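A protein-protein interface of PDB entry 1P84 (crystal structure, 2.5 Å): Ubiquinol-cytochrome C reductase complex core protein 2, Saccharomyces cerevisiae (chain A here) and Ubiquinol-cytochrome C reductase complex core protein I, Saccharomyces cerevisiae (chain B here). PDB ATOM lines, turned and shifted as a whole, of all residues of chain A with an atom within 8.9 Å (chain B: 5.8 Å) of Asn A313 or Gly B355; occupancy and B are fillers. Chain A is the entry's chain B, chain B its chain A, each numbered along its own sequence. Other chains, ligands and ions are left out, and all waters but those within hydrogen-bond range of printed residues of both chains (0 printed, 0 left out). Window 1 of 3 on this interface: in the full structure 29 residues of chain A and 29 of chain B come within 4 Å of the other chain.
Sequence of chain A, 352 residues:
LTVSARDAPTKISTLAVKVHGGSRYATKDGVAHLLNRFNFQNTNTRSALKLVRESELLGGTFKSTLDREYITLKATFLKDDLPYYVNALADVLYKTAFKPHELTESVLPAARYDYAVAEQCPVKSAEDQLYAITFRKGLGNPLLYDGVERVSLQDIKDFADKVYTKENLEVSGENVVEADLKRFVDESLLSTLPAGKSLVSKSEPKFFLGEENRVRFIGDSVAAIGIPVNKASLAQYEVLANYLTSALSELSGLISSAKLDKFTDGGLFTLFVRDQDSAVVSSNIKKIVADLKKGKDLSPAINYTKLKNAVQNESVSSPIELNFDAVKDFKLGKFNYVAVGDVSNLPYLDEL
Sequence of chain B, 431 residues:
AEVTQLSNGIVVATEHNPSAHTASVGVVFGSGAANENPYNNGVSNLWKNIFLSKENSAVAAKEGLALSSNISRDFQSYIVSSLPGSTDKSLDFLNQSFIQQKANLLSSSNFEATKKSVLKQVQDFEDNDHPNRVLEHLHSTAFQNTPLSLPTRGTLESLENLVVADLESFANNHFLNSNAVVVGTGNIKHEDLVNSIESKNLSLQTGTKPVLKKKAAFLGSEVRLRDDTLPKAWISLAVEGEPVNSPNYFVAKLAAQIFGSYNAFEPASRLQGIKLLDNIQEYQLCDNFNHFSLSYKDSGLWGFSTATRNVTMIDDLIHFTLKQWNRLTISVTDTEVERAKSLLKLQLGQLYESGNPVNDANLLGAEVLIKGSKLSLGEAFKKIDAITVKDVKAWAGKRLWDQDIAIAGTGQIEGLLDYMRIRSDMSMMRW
The side-chain amide oxygen (OD1) of Asn A313 sits close to the backbone carbonyl oxygen (O) of Ala B20, at 2.9 Å. O of Gly B355 lies within hydrogen-bond range of ND2 of Asn A313, at 2.9 Å.
O of Val A311 is in hydrogen-bond range of ND2 of Asn A313 (3.3 Å).
Leu A307 touches Thr B22 (CD2 to CG2, 3.9 Å). His B21 touches Ala A310 (CB to O, 3.8 Å). CB of His B21 touches OD1 of Asn A313, 3.7 Å away. Val A316 touches His B21 (CG1 to CE1, 3.98 Å).
Of the printed residues of chain B, Leu A307 touches Thr B22 (3.9 Å). Asn A313 touches just these residues of chain B: Ala B20 (2.9 Å), His B21 (3.7 Å) and Gly B355 (2.9 Å). Printed residues of chain A within 4 Å of Ala B20: Asn A313. Printed residues of chain A within 4 Å of His B21: Ala A310, Asn A313 and Val A316. Printed residues of chain A within 4 Å of Thr B22: Leu A307 (3.9 Å). Of the printed residues of chain A, Gly B355 touches Asn A313 (2.9 Å). The nearest residue of chain B that does not touch Asn A313 is Asn B356 (4.9 Å). The nearest printed residue of chain A that does not touch Gly B355 is Val A311 (4.001 Å). The nearest printed residue of chain B that does not touch Val A316 is Ala B20 (7.3 Å).
Hydrophobic or aromatic side chains of chain B within 4 Å of the printed part of chain A: His B21.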
ATOM      1  N   ARG A   6     -16.000  24.588  33.471  1.00  0.00           N
ATOM      2  CA  ARG A   6     -17.467  24.574  33.523  1.00  0.00           C
ATOM      3  C   ARG A   6     -17.952  24.453  34.967  1.00  0.00           C
ATOM      4  O   ARG A   6     -17.949  23.366  35.534  1.00  0.00           O
ATOM      5  CB  ARG A   6     -18.047  23.424  32.684  1.00  0.00           C
ATOM      6  CG  ARG A   6     -19.574  23.350  32.689  1.00  0.00           C
ATOM      7  CD  ARG A   6     -20.116  22.620  31.463  1.00  0.00           C
ATOM      8  NE  ARG A   6     -19.666  21.232  31.377  1.00  0.00           N
ATOM      9  CZ  ARG A   6     -19.093  20.690  30.302  1.00  0.00           C
ATOM     10  NH1 ARG A   6     -18.720  19.415  30.319  1.00  0.00           N
ATOM     11  NH2 ARG A   6     -18.879  21.422  29.214  1.00  0.00           N
ATOM     12  N   LYS A  18      -5.240  16.217  30.195  1.00  0.00           N
ATOM     13  CA  LYS A  18      -5.104  15.305  29.063  1.00  0.00           C
ATOM     14  C   LYS A  18      -3.773  15.600  28.394  1.00  0.00           C
ATOM     15  O   LYS A  18      -3.324  16.743  28.381  1.00  0.00           O
ATOM     16  CB  LYS A  18      -6.250  15.498  28.071  1.00  0.00           C
ATOM     17  CG  LYS A  18      -7.620  15.213  28.658  1.00  0.00           C
ATOM     18  CD  LYS A  18      -8.727  15.454  27.642  1.00  0.00           C
ATOM     19  CE  LYS A  18     -10.105  15.372  28.298  1.00  0.00           C
ATOM     20  NZ  LYS A  18     -11.214  15.694  27.348  1.00  0.00           N
ATOM     21  N   GLU A 174     -13.674  20.017  35.299  1.00  0.00           N
ATOM     22  CA  GLU A 174     -15.115  19.835  35.382  1.00  0.00           C
ATOM     23  C   GLU A 174     -15.589  20.342  36.740  1.00  0.00           C
ATOM     24  O   GLU A 174     -14.992  20.026  37.767  1.00  0.00           O
ATOM     25  CB  GLU A 174     -15.463  18.354  35.220  1.00  0.00           C
ATOM     26  CG  GLU A 174     -16.931  18.086  34.946  1.00  0.00           C
ATOM     27  CD  GLU A 174     -17.420  18.780  33.686  1.00  0.00           C
ATOM     28  OE1 GLU A 174     -16.869  18.511  32.592  1.00  0.00           O
ATOM     29  OE2 GLU A 174     -18.356  19.601  33.796  1.00  0.00           O
ATOM     30  N   LEU A 307     -29.182   9.584  21.198  1.00  0.00           N
ATOM     31  CA  LEU A 307     -29.450   9.575  22.636  1.00  0.00           C
ATOM     32  C   LEU A 307     -28.328   8.875  23.397  1.00  0.00           C
ATOM     33  O   LEU A 307     -27.911   9.332  24.462  1.00  0.00           O
ATOM     34  CB  LEU A 307     -30.798   8.890  22.917  1.00  0.00           C
ATOM     35  CG  LEU A 307     -31.321   8.644  24.341  1.00  0.00           C
ATOM     36  CD1 LEU A 307     -30.758   7.354  24.914  1.00  0.00           C
ATOM     37  CD2 LEU A 307     -31.031   9.830  25.245  1.00  0.00           C
ATOM     38  N   LYS A 308     -27.845   7.766  22.844  1.00  0.00           N
ATOM     39  CA  LYS A 308     -26.774   6.997  23.466  1.00  0.00           C
ATOM     40  C   LYS A 308     -25.444   7.747  23.365  1.00  0.00           C
ATOM     41  O   LYS A 308     -24.555   7.563  24.198  1.00  0.00           O
ATOM     42  CB  LYS A 308     -26.655   5.620  22.800  1.00  0.00           C
ATOM     43  CG  LYS A 308     -26.191   4.497  23.730  1.00  0.00           C
ATOM     44  CD  LYS A 308     -27.279   4.106  24.730  1.00  0.00           C
ATOM     45  CE  LYS A 308     -26.826   2.983  25.656  1.00  0.00           C
ATOM     46  NZ  LYS A 308     -25.695   3.396  26.541  1.00  0.00           N
ATOM     47  N   ASN A 309     -25.318   8.601  22.353  1.00  0.00           N
ATOM     48  CA  ASN A 309     -24.097   9.375  22.155  1.00  0.00           C
ATOM     49  C   ASN A 309     -24.145  10.708  22.905  1.00  0.00           C
ATOM     50  O   ASN A 309     -23.339  11.604  22.655  1.00  0.00           O
ATOM     51  CB  ASN A 309     -23.857   9.609  20.662  1.00  0.00           C
ATOM     52  CG  ASN A 309     -22.387   9.569  20.296  1.00  0.00           C
ATOM     53  OD1 ASN A 309     -21.889  10.437  19.582  1.00  0.00           O
ATOM     54  ND2 ASN A 309     -21.685   8.551  20.781  1.00  0.00           N
ATOM     55  N   ALA A 310     -25.095  10.820  23.828  1.00  0.00           N
ATOM     56  CA  ALA A 310     -25.267  12.023  24.634  1.00  0.00           C
ATOM     57  C   ALA A 310     -25.087  11.704  26.114  1.00  0.00           C
ATOM     58  O   ALA A 310     -24.725  12.578  26.902  1.00  0.00           O
ATOM     59  CB  ALA A 310     -26.640  12.632  24.392  1.00  0.00           C
ATOM     60  N   VAL A 311     -25.336  10.446  26.482  1.00  0.00           N
ATOM     61  CA  VAL A 311     -25.195   9.994  27.866  1.00  0.00           C
ATOM     62  C   VAL A 311     -23.745  10.121  28.326  1.00  0.00           C
ATOM     63  O   VAL A 311     -23.448   9.996  29.514  1.00  0.00           O
ATOM     64  CB  VAL A 311     -25.660   8.527  28.045  1.00  0.00           C
ATOM     65  CG1 VAL A 311     -27.122   8.387  27.661  1.00  0.00           C
ATOM     66  CG2 VAL A 311     -24.796   7.585  27.219  1.00  0.00           C
ATOM     67  N   GLN A 312     -22.856  10.362  27.366  1.00  0.00           N
ATOM     68  CA  GLN A 312     -21.435  10.531  27.632  1.00  0.00           C
ATOM     69  C   GLN A 312     -21.178  11.990  28.008  1.00  0.00           C
ATOM     70  O   GLN A 312     -20.824  12.813  27.161  1.00  0.00           O
ATOM     71  CB  GLN A 312     -20.629  10.133  26.394  1.00  0.00           C
ATOM     72  CG  GLN A 312     -20.887   8.701  25.948  1.00  0.00           C
ATOM     73  CD  GLN A 312     -20.208   8.355  24.642  1.00  0.00           C
ATOM     74  OE1 GLN A 312     -19.029   8.641  24.444  1.00  0.00           O
ATOM     75  NE2 GLN A 312     -20.953   7.729  23.740  1.00  0.00           N
ATOM     76  N   ASN A 313     -21.396  12.299  29.287  1.00  0.00           N
ATOM     77  CA  ASN A 313     -21.215  13.650  29.823  1.00  0.00           C
ATOM     78  C   ASN A 313     -19.764  14.051  30.079  1.00  0.00           C
ATOM     79  O   ASN A 313     -19.482  15.216  30.369  1.00  0.00           O
ATOM     80  CB  ASN A 313     -22.041  13.834  31.102  1.00  0.00           C
ATOM     81  CG  ASN A 313     -23.529  13.928  30.824  1.00  0.00           C
ATOM     82  OD1 ASN A 313     -24.023  14.962  30.374  1.00  0.00           O
ATOM     83  ND2 ASN A 313     -24.252  12.843  31.084  1.00  0.00           N
ATOM     84  N   GLU A 314     -18.850  13.086  30.012  1.00  0.00           N
ATOM     85  CA  GLU A 314     -17.435  13.377  30.213  1.00  0.00           C
ATOM     86  C   GLU A 314     -16.835  13.780  28.865  1.00  0.00           C
ATOM     87  O   GLU A 314     -15.750  14.363  28.799  1.00  0.00           O
ATOM     88  CB  GLU A 314     -16.708  12.157  30.802  1.00  0.00           C
ATOM     89  CG  GLU A 314     -16.542  10.954  29.863  1.00  0.00           C
ATOM     90  CD  GLU A 314     -15.212  10.960  29.115  1.00  0.00           C
ATOM     91  OE1 GLU A 314     -15.222  11.030  27.868  1.00  0.00           O
ATOM     92  OE2 GLU A 314     -14.152  10.887  29.774  1.00  0.00           O
ATOM     93  N   SER A 315     -17.574  13.485  27.798  1.00  0.00           N
ATOM     94  CA  SER A 315     -17.155  13.788  26.435  1.00  0.00           C
ATOM     95  C   SER A 315     -17.893  15.000  25.860  1.00  0.00           C
ATOM     96  O   SER A 315     -18.393  14.953  24.732  1.00  0.00           O
ATOM     97  CB  SER A 315     -17.373  12.561  25.540  1.00  0.00           C
ATOM     98  OG  SER A 315     -16.918  12.788  24.215  1.00  0.00           O
ATOM     99  N   VAL A 316     -17.977  16.078  26.639  1.00  0.00           N
ATOM    100  CA  VAL A 316     -18.641  17.294  26.170  1.00  0.00           C
ATOM    101  C   VAL A 316     -17.612  18.131  25.403  1.00  0.00           C
ATOM    102  O   VAL A 316     -17.333  19.288  25.736  1.00  0.00           O
ATOM    103  CB  VAL A 316     -19.267  18.106  27.334  1.00  0.00           C
ATOM    104  CG1 VAL A 316     -20.080  19.277  26.786  1.00  0.00           C
ATOM    105  CG2 VAL A 316     -20.163  17.211  28.175  1.00  0.00           C
ATOM    106  N   SER A 317     -17.028  17.494  24.393  1.00  0.00           N
ATOM    107  CA  SER A 317     -16.019  18.085  23.518  1.00  0.00           C
ATOM    108  C   SER A 317     -15.861  17.163  22.305  1.00  0.00           C
ATOM    109  O   SER A 317     -14.845  17.196  21.609  1.00  0.00           O
ATOM    110  CB  SER A 317     -14.682  18.236  24.262  1.00  0.00           C
ATOM    111  OG  SER A 317     -14.251  17.007  24.826  1.00  0.00           O
ATOM    112  N   SER A 318     -16.892  16.354  22.067  1.00  0.00           N
ATOM    113  CA  SER A 318     -16.932  15.396  20.963  1.00  0.00           C
ATOM    114  C   SER A 318     -16.976  16.083  19.596  1.00  0.00           C
ATOM    115  O   SER A 318     -17.474  17.203  19.473  1.00  0.00           O
ATOM    116  CB  SER A 318     -18.150  14.475  21.113  1.00  0.00           C
ATOM    117  OG  SER A 318     -19.364  15.204  21.013  1.00  0.00           O
ATOM    118  N   ALA B  20     -27.330  18.793  31.648  1.00  0.00           N
ATOM    119  CA  ALA B  20     -27.451  17.350  31.803  1.00  0.00           C
ATOM    120  C   ALA B  20     -27.349  16.580  30.496  1.00  0.00           C
ATOM    121  O   ALA B  20     -26.858  15.449  30.489  1.00  0.00           O
ATOM    122  CB  ALA B  20     -28.758  17.009  32.503  1.00  0.00           C
ATOM    123  N   HIS B  21     -27.818  17.190  29.405  1.00  0.00           N
ATOM    124  CA  HIS B  21     -27.812  16.573  28.074  1.00  0.00           C
ATOM    125  C   HIS B  21     -28.957  15.580  27.882  1.00  0.00           C
ATOM    126  O   HIS B  21     -29.492  15.458  26.782  1.00  0.00           O
ATOM    127  CB  HIS B  21     -26.484  15.860  27.775  1.00  0.00           C
ATOM    128  CG  HIS B  21     -25.471  16.713  27.080  1.00  0.00           C
ATOM    129  ND1 HIS B  21     -24.793  17.735  27.711  1.00  0.00           N
ATOM    130  CD2 HIS B  21     -24.989  16.670  25.815  1.00  0.00           C
ATOM    131  CE1 HIS B  21     -23.937  18.280  26.866  1.00  0.00           C
ATOM    132  NE2 HIS B  21     -24.036  17.651  25.708  1.00  0.00           N
ATOM    133  N   THR B  22     -29.300  14.846  28.938  1.00  0.00           N
ATOM    134  CA  THR B  22     -30.381  13.861  28.881  1.00  0.00           C
ATOM    135  C   THR B  22     -31.341  14.004  30.061  1.00  0.00           C
ATOM    136  O   THR B  22     -31.173  14.875  30.920  1.00  0.00           O
ATOM    137  CB  THR B  22     -29.846  12.396  28.848  1.00  0.00           C
ATOM    138  OG1 THR B  22     -29.059  12.137  30.018  1.00  0.00           O
ATOM    139  CG2 THR B  22     -29.001  12.148  27.605  1.00  0.00           C
ATOM    140  N   GLU B 353     -23.828  12.529  43.008  1.00  0.00           N
ATOM    141  CA  GLU B 353     -23.656  13.421  41.869  1.00  0.00           C
ATOM    142  C   GLU B 353     -22.689  12.982  40.777  1.00  0.00           C
ATOM    143  O   GLU B 353     -21.569  13.481  40.672  1.00  0.00           O
ATOM    144  CB  GLU B 353     -23.360  14.865  42.317  1.00  0.00           C
ATOM    145  CG  GLU B 353     -22.225  15.037  43.301  1.00  0.00           C
ATOM    146  CD  GLU B 353     -21.903  16.495  43.569  1.00  0.00           C
ATOM    147  OE1 GLU B 353     -20.849  16.957  43.091  1.00  0.00           O
ATOM    148  OE2 GLU B 353     -22.694  17.176  44.255  1.00  0.00           O
ATOM    149  N   SER B 354     -23.151  12.046  39.957  1.00  0.00           N
ATOM    150  CA  SER B 354     -22.375  11.553  38.829  1.00  0.00           C
ATOM    151  C   SER B 354     -23.052  12.075  37.560  1.00  0.00           C
ATOM    152  O   SER B 354     -24.106  12.722  37.627  1.00  0.00           O
ATOM    153  CB  SER B 354     -22.362  10.024  38.810  1.00  0.00           C
ATOM    154  OG  SER B 354     -21.603   9.539  37.714  1.00  0.00           O
ATOM    155  N   GLY B 355     -22.448  11.797  36.405  1.00  0.00           N
ATOM    156  CA  GLY B 355     -23.025  12.242  35.146  1.00  0.00           C
ATOM    157  C   GLY B 355     -24.005  11.244  34.548  1.00  0.00           C
ATOM    158  O   GLY B 355     -24.039  11.054  33.327  1.00  0.00           O
ATOM    159  N   ASN B 356     -24.802  10.604  35.402  1.00  0.00           N
ATOM    160  CA  ASN B 356     -25.775   9.618  34.947  1.00  0.00           C
ATOM    161  C   ASN B 356     -27.079   9.720  35.727  1.00  0.00           C
ATOM    162  O   ASN B 356     -27.152   9.344  36.899  1.00  0.00           O
ATOM    163  CB  ASN B 356     -25.203   8.203  35.059  1.00  0.00           C
ATOM    164  CG  ASN B 356     -26.024   7.179  34.295  1.00  0.00           C
ATOM    165  OD1 ASN B 356     -27.152   7.449  33.879  1.00  0.00           O
ATOM    166  ND2 ASN B 356     -25.452   5.996  34.094  1.00  0.00           N
ATOM    167  N   PRO B 357     -28.134  10.225  35.069  1.00  0.00           N
ATOM    168  CA  PRO B 357     -29.477  10.411  35.630  1.00  0.00           C
ATOM    169  C   PRO B 357     -30.157   9.143  36.151  1.00  0.00           C
ATOM    170  O   PRO B 357     -30.954   9.215  37.088  1.00  0.00           O
ATOM    171  CB  PRO B 357     -30.250  11.015  34.457  1.00  0.00           C
ATOM    172  CG  PRO B 357     -29.198  11.788  33.732  1.00  0.00           C
ATOM    173  CD  PRO B 357     -28.058  10.804  33.717  1.00  0.00           C
